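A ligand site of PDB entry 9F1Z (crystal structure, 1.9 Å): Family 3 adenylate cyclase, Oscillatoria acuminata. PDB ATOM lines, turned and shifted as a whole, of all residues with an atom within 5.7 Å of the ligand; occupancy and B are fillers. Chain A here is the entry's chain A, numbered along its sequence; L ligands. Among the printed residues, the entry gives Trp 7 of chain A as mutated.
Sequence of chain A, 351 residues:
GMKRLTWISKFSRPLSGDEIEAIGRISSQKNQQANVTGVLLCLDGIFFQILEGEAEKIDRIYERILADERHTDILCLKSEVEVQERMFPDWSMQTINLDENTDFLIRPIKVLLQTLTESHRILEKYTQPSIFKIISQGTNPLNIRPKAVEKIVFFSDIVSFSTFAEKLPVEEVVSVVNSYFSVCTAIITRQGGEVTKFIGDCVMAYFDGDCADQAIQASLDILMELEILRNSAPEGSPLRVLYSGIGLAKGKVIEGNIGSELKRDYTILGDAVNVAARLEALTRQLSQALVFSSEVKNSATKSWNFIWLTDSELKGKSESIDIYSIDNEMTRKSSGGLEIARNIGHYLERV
OG of Ser 27 lies within hydrogen-bond range of O of Ile 23, 2.7 Å away. SD of Met 93 lies within hydrogen-bond range of N of Leu 40. The side-chain carboxylate of Asp 68 is in salt-bridge range of the guanidinium group of Arg 70 (2.6 Å). O of Asn 31 is in hydrogen-bond range of N of Val 36 (2.8 Å). The backbone carbonyl oxygen (O) of Ile 65 lies within hydrogen-bond range of a ring nitrogen (NE2) of His 71, 2.7 Å away. A ring nitrogen (ND1) of His 71 sits at hydrogen-bond distance from the side-chain hydroxyl (OG) of Ser 9 (2.8 Å). The backbone NH (N) of Ser 9 is in hydrogen-bond range of the backbone carbonyl oxygen (O) of Phe 47 (2.9 Å). ND2 of Asn 31 sits close to O of Ser 27.
CH2 of Trp 7 touches C7 of the ligand (3.5 Å). CG2 of Ile 23 touches C8 of the ligand (3.6 Å). Lys 30 touches the ligand (CD to O7, 3.0 Å). CG of Phe 47 touches C7 of the ligand, at 3.5 Å. Leu 51 touches the ligand. Ile 61 touches the ligand (CG2 to N2, 3.3 Å). CA of Ile 65 touches O3 of the ligand, 3.7 Å away. NH2 of Arg 70 touches O4 of the ligand, at 3.6 Å. His 71 touches the ligand (ND1 to C7, 3.9 Å). Met 93 touches the ligand (CE to O2, 3.7 Å). Hydrophobic or aromatic side chains that line the ligand: Trp 7, Ile 23, Phe 47, Leu 51, Ile 61, Ile 65, His 71 and Met 93.
The guanidinium group of Arg 64 lies within salt-bridge range of an oxygen (O7) of the ligand. A nitrogen (N3) of the ligand sits close to the side-chain hydroxyl (OG) of Ser 27 (3.2 Å). O of Arg 64 is in hydrogen-bond range of O3 of the ligand (3.4 Å). NE2 of Gln 49 sits at hydrogen-bond distance from N3 of the ligand (3.1 Å). An oxygen (O3) of the ligand sits at hydrogen-bond distance from the side-chain carboxylate (OD2) of Asp 68, 2.8 Å away. The side-chain amide oxygen of Asn 31 is in hydrogen-bond range of a nitrogen (N2) of the ligand.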
ATOM      1  N   TRP A   7     -12.617   5.925 -29.525  1.00  0.00           N
ATOM      2  CA  TRP A   7     -13.028   6.045 -28.139  1.00  0.00           C
ATOM      3  C   TRP A   7     -14.415   6.660 -28.038  1.00  0.00           C
ATOM      4  O   TRP A   7     -14.922   7.264 -28.984  1.00  0.00           O
ATOM      5  CB  TRP A   7     -12.022   6.860 -27.295  1.00  0.00           C
ATOM      6  CG  TRP A   7     -11.735   8.247 -27.816  1.00  0.00           C
ATOM      7  CD1 TRP A   7     -10.727   8.629 -28.659  1.00  0.00           C
ATOM      8  CD2 TRP A   7     -12.499   9.423 -27.549  1.00  0.00           C
ATOM      9  NE1 TRP A   7     -10.807   9.981 -28.902  1.00  0.00           N
ATOM     10  CE2 TRP A   7     -11.895  10.496 -28.228  1.00  0.00           C
ATOM     11  CE3 TRP A   7     -13.650   9.663 -26.790  1.00  0.00           C
ATOM     12  CZ2 TRP A   7     -12.397  11.798 -28.187  1.00  0.00           C
ATOM     13  CZ3 TRP A   7     -14.145  10.968 -26.736  1.00  0.00           C
ATOM     14  CH2 TRP A   7     -13.523  12.020 -27.437  1.00  0.00           C
ATOM     15  N   SER A   9     -17.145   8.610 -24.994  1.00  0.00           N
ATOM     16  CA  SER A   9     -17.215   9.268 -23.687  1.00  0.00           C
ATOM     17  C   SER A   9     -18.621   9.781 -23.471  1.00  0.00           C
ATOM     18  O   SER A   9     -19.506   9.631 -24.313  1.00  0.00           O
ATOM     19  CB  SER A   9     -16.230  10.445 -23.564  1.00  0.00           C
ATOM     20  OG  SER A   9     -16.556  11.481 -24.464  1.00  0.00           O
ATOM     21  N   ILE A  23     -16.148  22.521 -30.336  1.00  0.00           N
ATOM     22  CA  ILE A  23     -15.205  21.426 -30.088  1.00  0.00           C
ATOM     23  C   ILE A  23     -14.639  20.920 -31.407  1.00  0.00           C
ATOM     24  O   ILE A  23     -13.419  20.788 -31.566  1.00  0.00           O
ATOM     25  CB  ILE A  23     -15.887  20.303 -29.275  1.00  0.00           C
ATOM     26  CG1 ILE A  23     -16.189  20.792 -27.848  1.00  0.00           C
ATOM     27  CG2 ILE A  23     -15.014  19.054 -29.224  1.00  0.00           C
ATOM     28  CD1 ILE A  23     -17.131  19.861 -27.084  1.00  0.00           C
ATOM     29  N   ILE A  26     -11.935  23.521 -33.060  1.00  0.00           N
ATOM     30  CA  ILE A  26     -10.563  23.551 -32.560  1.00  0.00           C
ATOM     31  C   ILE A  26      -9.900  22.202 -32.784  1.00  0.00           C
ATOM     32  O   ILE A  26      -8.711  22.131 -33.118  1.00  0.00           O
ATOM     33  CB  ILE A  26     -10.452  23.999 -31.084  1.00  0.00           C
ATOM     34  CG1 ILE A  26     -11.141  25.323 -30.791  1.00  0.00           C
ATOM     35  CG2 ILE A  26      -8.983  24.198 -30.679  1.00  0.00           C
ATOM     36  CD1 ILE A  26     -12.457  25.207 -30.095  1.00  0.00           C
ATOM     37  N   SER A  27     -10.653  21.096 -32.622  1.00  0.00           N
ATOM     38  CA  SER A  27     -10.089  19.785 -32.923  1.00  0.00           C
ATOM     39  C   SER A  27      -9.557  19.738 -34.341  1.00  0.00           C
ATOM     40  O   SER A  27      -8.456  19.241 -34.585  1.00  0.00           O
ATOM     41  CB  SER A  27     -11.137  18.678 -32.718  1.00  0.00           C
ATOM     42  OG  SER A  27     -11.648  18.729 -31.395  1.00  0.00           O
ATOM     43  N   SER A  28     -10.321  20.284 -35.284  1.00  0.00           N
ATOM     44  CA  SER A  28      -9.886  20.256 -36.678  1.00  0.00           C
ATOM     45  C   SER A  28      -8.626  21.081 -36.854  1.00  0.00           C
ATOM     46  O   SER A  28      -7.665  20.656 -37.521  1.00  0.00           O
ATOM     47  CB  SER A  28     -11.006  20.764 -37.595  1.00  0.00           C
ATOM     48  OG  SER A  28     -10.597  20.693 -38.957  1.00  0.00           O
ATOM     49  N   LYS A  30      -6.291  22.020 -34.560  1.00  0.00           N
ATOM     50  CA  LYS A  30      -5.154  21.330 -33.931  1.00  0.00           C
ATOM     51  C   LYS A  30      -4.723  20.091 -34.708  1.00  0.00           C
ATOM     52  O   LYS A  30      -3.527  19.837 -34.893  1.00  0.00           O
ATOM     53  CB  LYS A  30      -5.493  20.949 -32.491  1.00  0.00           C
ATOM     54  CG  LYS A  30      -5.866  22.092 -31.561  1.00  0.00           C
ATOM     55  CD  LYS A  30      -4.861  23.219 -31.609  1.00  0.00           C
ATOM     56  CE  LYS A  30      -5.523  24.598 -31.645  1.00  0.00           C
ATOM     57  NZ  LYS A  30      -4.775  25.655 -32.415  1.00  0.00           N
ATOM     58  N   ASN A  31      -5.677  19.263 -35.145  1.00  0.00           N
ATOM     59  CA  ASN A  31      -5.272  18.058 -35.850  1.00  0.00           C
ATOM     60  C   ASN A  31      -4.619  18.389 -37.186  1.00  0.00           C
ATOM     61  O   ASN A  31      -3.698  17.673 -37.621  1.00  0.00           O
ATOM     62  CB  ASN A  31      -6.466  17.108 -36.042  1.00  0.00           C
ATOM     63  CG  ASN A  31      -6.935  16.490 -34.734  1.00  0.00           C
ATOM     64  OD1 ASN A  31      -6.264  16.621 -33.700  1.00  0.00           O
ATOM     65  ND2 ASN A  31      -8.077  15.805 -34.758  1.00  0.00           N
ATOM     66  N   VAL A  36      -3.088  15.015 -38.250  1.00  0.00           N
ATOM     67  CA  VAL A  36      -3.945  13.984 -37.665  1.00  0.00           C
ATOM     68  C   VAL A  36      -5.320  14.125 -38.324  1.00  0.00           C
ATOM     69  O   VAL A  36      -5.764  15.243 -38.600  1.00  0.00           O
ATOM     70  CB  VAL A  36      -4.037  14.165 -36.137  1.00  0.00           C
ATOM     71  CG1 VAL A  36      -5.334  13.590 -35.579  1.00  0.00           C
ATOM     72  CG2 VAL A  36      -2.777  13.619 -35.426  1.00  0.00           C
ATOM     73  N   LEU A  40     -15.613  12.879 -35.415  1.00  0.00           N
ATOM     74  CA  LEU A  40     -16.206  12.966 -34.087  1.00  0.00           C
ATOM     75  C   LEU A  40     -17.708  13.028 -34.245  1.00  0.00           C
ATOM     76  O   LEU A  40     -18.218  13.865 -34.987  1.00  0.00           O
ATOM     77  CB  LEU A  40     -15.667  14.201 -33.338  1.00  0.00           C
ATOM     78  CG  LEU A  40     -16.469  14.655 -32.110  1.00  0.00           C
ATOM     79  CD1 LEU A  40     -16.257  13.668 -30.979  1.00  0.00           C
ATOM     80  CD2 LEU A  40     -16.077  16.062 -31.671  1.00  0.00           C
ATOM     81  N   PHE A  47     -20.036  11.108 -26.858  1.00  0.00           N
ATOM     82  CA  PHE A  47     -19.090  11.412 -27.911  1.00  0.00           C
ATOM     83  C   PHE A  47     -18.472  10.103 -28.398  1.00  0.00           C
ATOM     84  O   PHE A  47     -18.190   9.213 -27.596  1.00  0.00           O
ATOM     85  CB  PHE A  47     -17.957  12.337 -27.421  1.00  0.00           C
ATOM     86  CG  PHE A  47     -18.351  13.799 -27.267  1.00  0.00           C
ATOM     87  CD1 PHE A  47     -18.716  14.560 -28.372  1.00  0.00           C
ATOM     88  CD2 PHE A  47     -18.262  14.428 -26.039  1.00  0.00           C
ATOM     89  CE1 PHE A  47     -19.048  15.919 -28.238  1.00  0.00           C
ATOM     90  CE2 PHE A  47     -18.579  15.788 -25.896  1.00  0.00           C
ATOM     91  CZ  PHE A  47     -18.975  16.531 -26.990  1.00  0.00           C
ATOM     92  N   GLN A  49     -15.264   9.081 -31.181  1.00  0.00           N
ATOM     93  CA  GLN A  49     -14.282   9.650 -32.099  1.00  0.00           C
ATOM     94  C   GLN A  49     -13.316   8.575 -32.586  1.00  0.00           C
ATOM     95  O   GLN A  49     -12.981   7.646 -31.845  1.00  0.00           O
ATOM     96  CB  GLN A  49     -13.522  10.827 -31.472  1.00  0.00           C
ATOM     97  CG  GLN A  49     -12.267  11.256 -32.245  1.00  0.00           C
ATOM     98  CD  GLN A  49     -11.493  12.364 -31.544  1.00  0.00           C
ATOM     99  OE1 GLN A  49     -10.448  12.104 -30.937  1.00  0.00           O
ATOM    100  NE2 GLN A  49     -11.949  13.610 -31.686  1.00  0.00           N
ATOM    101  N   LEU A  51      -9.525   8.670 -34.324  1.00  0.00           N
ATOM    102  CA  LEU A  51      -8.372   9.562 -34.400  1.00  0.00           C
ATOM    103  C   LEU A  51      -7.195   8.757 -34.903  1.00  0.00           C
ATOM    104  O   LEU A  51      -6.912   7.669 -34.368  1.00  0.00           O
ATOM    105  CB  LEU A  51      -8.064  10.152 -33.011  1.00  0.00           C
ATOM    106  CG  LEU A  51      -7.338  11.475 -32.806  1.00  0.00           C
ATOM    107  CD1 LEU A  51      -8.111  12.658 -33.336  1.00  0.00           C
ATOM    108  CD2 LEU A  51      -7.090  11.648 -31.318  1.00  0.00           C
ATOM    109  N   ILE A  61      -2.213  14.403 -28.207  1.00  0.00           N
ATOM    110  CA  ILE A  61      -3.596  14.831 -28.393  1.00  0.00           C
ATOM    111  C   ILE A  61      -4.517  14.071 -27.465  1.00  0.00           C
ATOM    112  O   ILE A  61      -5.399  14.649 -26.809  1.00  0.00           O
ATOM    113  CB  ILE A  61      -4.020  14.643 -29.864  1.00  0.00           C
ATOM    114  CG1 ILE A  61      -3.068  15.374 -30.811  1.00  0.00           C
ATOM    115  CG2 ILE A  61      -5.452  15.101 -30.023  1.00  0.00           C
ATOM    116  CD1 ILE A  61      -3.663  15.694 -32.129  1.00  0.00           C
ATOM    117  N   ARG A  64      -4.412  15.247 -23.940  1.00  0.00           N
ATOM    118  CA  ARG A  64      -5.239  16.452 -23.834  1.00  0.00           C
ATOM    119  C   ARG A  64      -6.726  16.135 -23.753  1.00  0.00           C
ATOM    120  O   ARG A  64      -7.454  16.740 -22.957  1.00  0.00           O
ATOM    121  CB  ARG A  64      -4.970  17.375 -25.020  1.00  0.00           C
ATOM    122  CG  ARG A  64      -4.111  18.565 -24.701  1.00  0.00           C
ATOM    123  CD  ARG A  64      -4.060  19.524 -25.884  1.00  0.00           C
ATOM    124  NE  ARG A  64      -3.018  19.113 -26.826  1.00  0.00           N
ATOM    125  CZ  ARG A  64      -3.148  19.063 -28.142  1.00  0.00           C
ATOM    126  NH1 ARG A  64      -4.307  19.295 -28.740  1.00  0.00           N
ATOM    127  NH2 ARG A  64      -2.084  18.762 -28.874  1.00  0.00           N
ATOM    128  N   ILE A  65      -7.208  15.203 -24.591  1.00  0.00           N
ATOM    129  CA  ILE A  65      -8.633  14.905 -24.621  1.00  0.00           C
ATOM    130  C   ILE A  65      -9.094  14.361 -23.277  1.00  0.00           C
ATOM    131  O   ILE A  65     -10.194  14.673 -22.805  1.00  0.00           O
ATOM    132  CB  ILE A  65      -8.969  13.925 -25.763  1.00  0.00           C
ATOM    133  CG1 ILE A  65      -8.793  14.570 -27.149  1.00  0.00           C
ATOM    134  CG2 ILE A  65     -10.372  13.373 -25.611  1.00  0.00           C
ATOM    135  CD1 ILE A  65      -8.601  13.529 -28.299  1.00  0.00           C
ATOM    136  N   LEU A  66      -8.270  13.520 -22.652  1.00  0.00           N
ATOM    137  CA  LEU A  66      -8.633  12.958 -21.356  1.00  0.00           C
ATOM    138  C   LEU A  66      -8.814  14.023 -20.283  1.00  0.00           C
ATOM    139  O   LEU A  66      -9.549  13.790 -19.308  1.00  0.00           O
ATOM    140  CB  LEU A  66      -7.565  11.944 -20.930  1.00  0.00           C
ATOM    141  CG  LEU A  66      -7.419  10.699 -21.824  1.00  0.00           C
ATOM    142  CD1 LEU A  66      -6.070  10.049 -21.603  1.00  0.00           C
ATOM    143  CD2 LEU A  66      -8.537   9.696 -21.570  1.00  0.00           C
ATOM    144  N   ALA A  67      -8.228  15.205 -20.445  1.00  0.00           N
ATOM    145  CA  ALA A  67      -8.305  16.271 -19.460  1.00  0.00           C
ATOM    146  C   ALA A  67      -9.402  17.293 -19.741  1.00  0.00           C
ATOM    147  O   ALA A  67      -9.602  18.201 -18.926  1.00  0.00           O
ATOM    148  CB  ALA A  67      -6.959  16.993 -19.357  1.00  0.00           C
ATOM    149  N   ASP A  68     -10.104  17.192 -20.871  1.00  0.00           N
ATOM    150  CA  ASP A  68     -11.150  18.164 -21.193  1.00  0.00           C
ATOM    151  C   ASP A  68     -12.285  18.083 -20.168  1.00  0.00           C
ATOM    152  O   ASP A  68     -12.803  17.001 -19.884  1.00  0.00           O
ATOM    153  CB  ASP A  68     -11.697  17.920 -22.594  1.00  0.00           C
ATOM    154  CG  ASP A  68     -12.241  19.171 -23.237  1.00  0.00           C
ATOM    155  OD1 ASP A  68     -13.359  19.591 -22.862  1.00  0.00           O
ATOM    156  OD2 ASP A  68     -11.580  19.696 -24.171  1.00  0.00           O
ATOM    157  N   ARG A  70     -15.229  19.049 -20.575  1.00  0.00           N
ATOM    158  CA  ARG A  70     -16.531  18.914 -21.214  1.00  0.00           C
ATOM    159  C   ARG A  70     -16.982  17.465 -21.392  1.00  0.00           C
ATOM    160  O   ARG A  70     -18.119  17.228 -21.818  1.00  0.00           O
ATOM    161  CB  ARG A  70     -16.478  19.655 -22.563  1.00  0.00           C
ATOM    162  CG  ARG A  70     -16.299  21.168 -22.367  1.00  0.00           C
ATOM    163  CD  ARG A  70     -15.947  21.887 -23.651  1.00  0.00           C
ATOM    164  NE  ARG A  70     -14.638  21.483 -24.149  1.00  0.00           N
ATOM    165  CZ  ARG A  70     -13.976  22.128 -25.101  1.00  0.00           C
ATOM    166  NH1 ARG A  70     -14.472  23.211 -25.676  1.00  0.00           N
ATOM    167  NH2 ARG A  70     -12.785  21.674 -25.476  1.00  0.00           N
ATOM    168  N   HIS A  71     -16.156  16.485 -21.032  1.00  0.00           N
ATOM    169  CA  HIS A  71     -16.623  15.111 -21.063  1.00  0.00           C
ATOM    170  C   HIS A  71     -15.889  14.287 -20.010  1.00  0.00           C
ATOM    171  O   HIS A  71     -14.910  14.731 -19.406  1.00  0.00           O
ATOM    172  CB  HIS A  71     -16.469  14.477 -22.460  1.00  0.00           C
ATOM    173  CG  HIS A  71     -15.044  14.308 -22.900  1.00  0.00           C
ATOM    174  ND1 HIS A  71     -14.678  13.482 -23.936  1.00  0.00           N
ATOM    175  CD2 HIS A  71     -13.896  14.871 -22.453  1.00  0.00           C
ATOM    176  CE1 HIS A  71     -13.371  13.534 -24.100  1.00  0.00           C
ATOM    177  NE2 HIS A  71     -12.873  14.374 -23.218  1.00  0.00           N
ATOM    178  N   MET A  93     -10.678  16.927 -38.568  1.00  0.00           N
ATOM    179  CA  MET A  93     -11.657  16.384 -37.632  1.00  0.00           C
ATOM    180  C   MET A  93     -13.018  16.757 -38.210  1.00  0.00           C
ATOM    181  O   MET A  93     -13.375  17.935 -38.219  1.00  0.00           O
ATOM    182  CB  MET A  93     -11.479  16.964 -36.228  1.00  0.00           C
ATOM    183  CG  MET A  93     -12.248  16.232 -35.094  1.00  0.00           C
ATOM    184  SD  MET A  93     -12.557  14.452 -35.366  1.00  0.00           S
ATOM    185  CE  MET A  93     -10.941  13.869 -34.903  1.00  0.00           C
HETATM  186  N1  LIG L   1      -8.309  18.371 -29.452  1.00  0.00           N
HETATM  187  C1  LIG L   1      -7.472  18.048 -30.499  1.00  0.00           C
HETATM  188  O1  LIG L   1      -6.428  18.661 -30.668  1.00  0.00           O
HETATM  189  N2  LIG L   1      -7.806  17.032 -31.373  1.00  0.00           N
HETATM  190  C2  LIG L   1      -8.978  16.312 -31.194  1.00  0.00           C
HETATM  191  O2  LIG L   1      -9.269  15.412 -31.977  1.00  0.00           O
HETATM  192  C3  LIG L   1      -9.821  16.631 -30.135  1.00  0.00           C
HETATM  193  N3  LIG L   1     -10.985  15.928 -29.947  1.00  0.00           N
HETATM  194  C4  LIG L   1     -11.818  16.245 -28.893  1.00  0.00           C
HETATM  195  C5  LIG L   1     -13.009  15.546 -28.691  1.00  0.00           C
HETATM  196  C6  LIG L   1     -13.848  15.873 -27.628  1.00  0.00           C
HETATM  197  C7  LIG L   1     -15.128  15.115 -27.424  1.00  0.00           C
HETATM  198  C8  LIG L   1     -13.502  16.895 -26.754  1.00  0.00           C
HETATM  199  C9  LIG L   1     -14.412  17.252 -25.618  1.00  0.00           C
HETATM  200  C10 LIG L   1     -12.322  17.601 -26.959  1.00  0.00           C
HETATM  201  C11 LIG L   1     -11.480  17.282 -28.018  1.00  0.00           C
HETATM  202  N4  LIG L   1     -10.308  17.971 -28.207  1.00  0.00           N
HETATM  203  C12 LIG L   1      -9.473  17.667 -29.264  1.00  0.00           C
HETATM  204  C13 LIG L   1      -9.991  19.124 -27.280  1.00  0.00           C
HETATM  205  C14 LIG L   1      -8.793  19.030 -26.381  1.00  0.00           C
HETATM  206  O3  LIG L   1      -9.318  18.457 -25.200  1.00  0.00           O
HETATM  207  C15 LIG L   1      -8.230  20.463 -26.154  1.00  0.00           C
HETATM  208  O4  LIG L   1      -9.247  21.301 -25.661  1.00  0.00           O
HETATM  209  C16 LIG L   1      -7.676  21.104 -27.438  1.00  0.00           C
HETATM  210  O5  LIG L   1      -6.819  20.207 -28.118  1.00  0.00           O
HETATM  211  C17 LIG L   1      -6.932  22.436 -27.220  1.00  0.00           C
HETATM  212  O6  LIG L   1      -5.566  22.237 -26.854  1.00  0.00           O
HETATM  213  P1  LIG L   1      -4.357  23.253 -27.273  1.00  0.00           P
HETATM  214  O7  LIG L   1      -4.005  23.002 -28.729  1.00  0.00           O
HETATM  215  O8  LIG L   1      -4.730  24.719 -27.099  1.00  0.00           O
HETATM  216  O9  LIG L   1      -3.121  22.995 -26.440  1.00  0.00           O
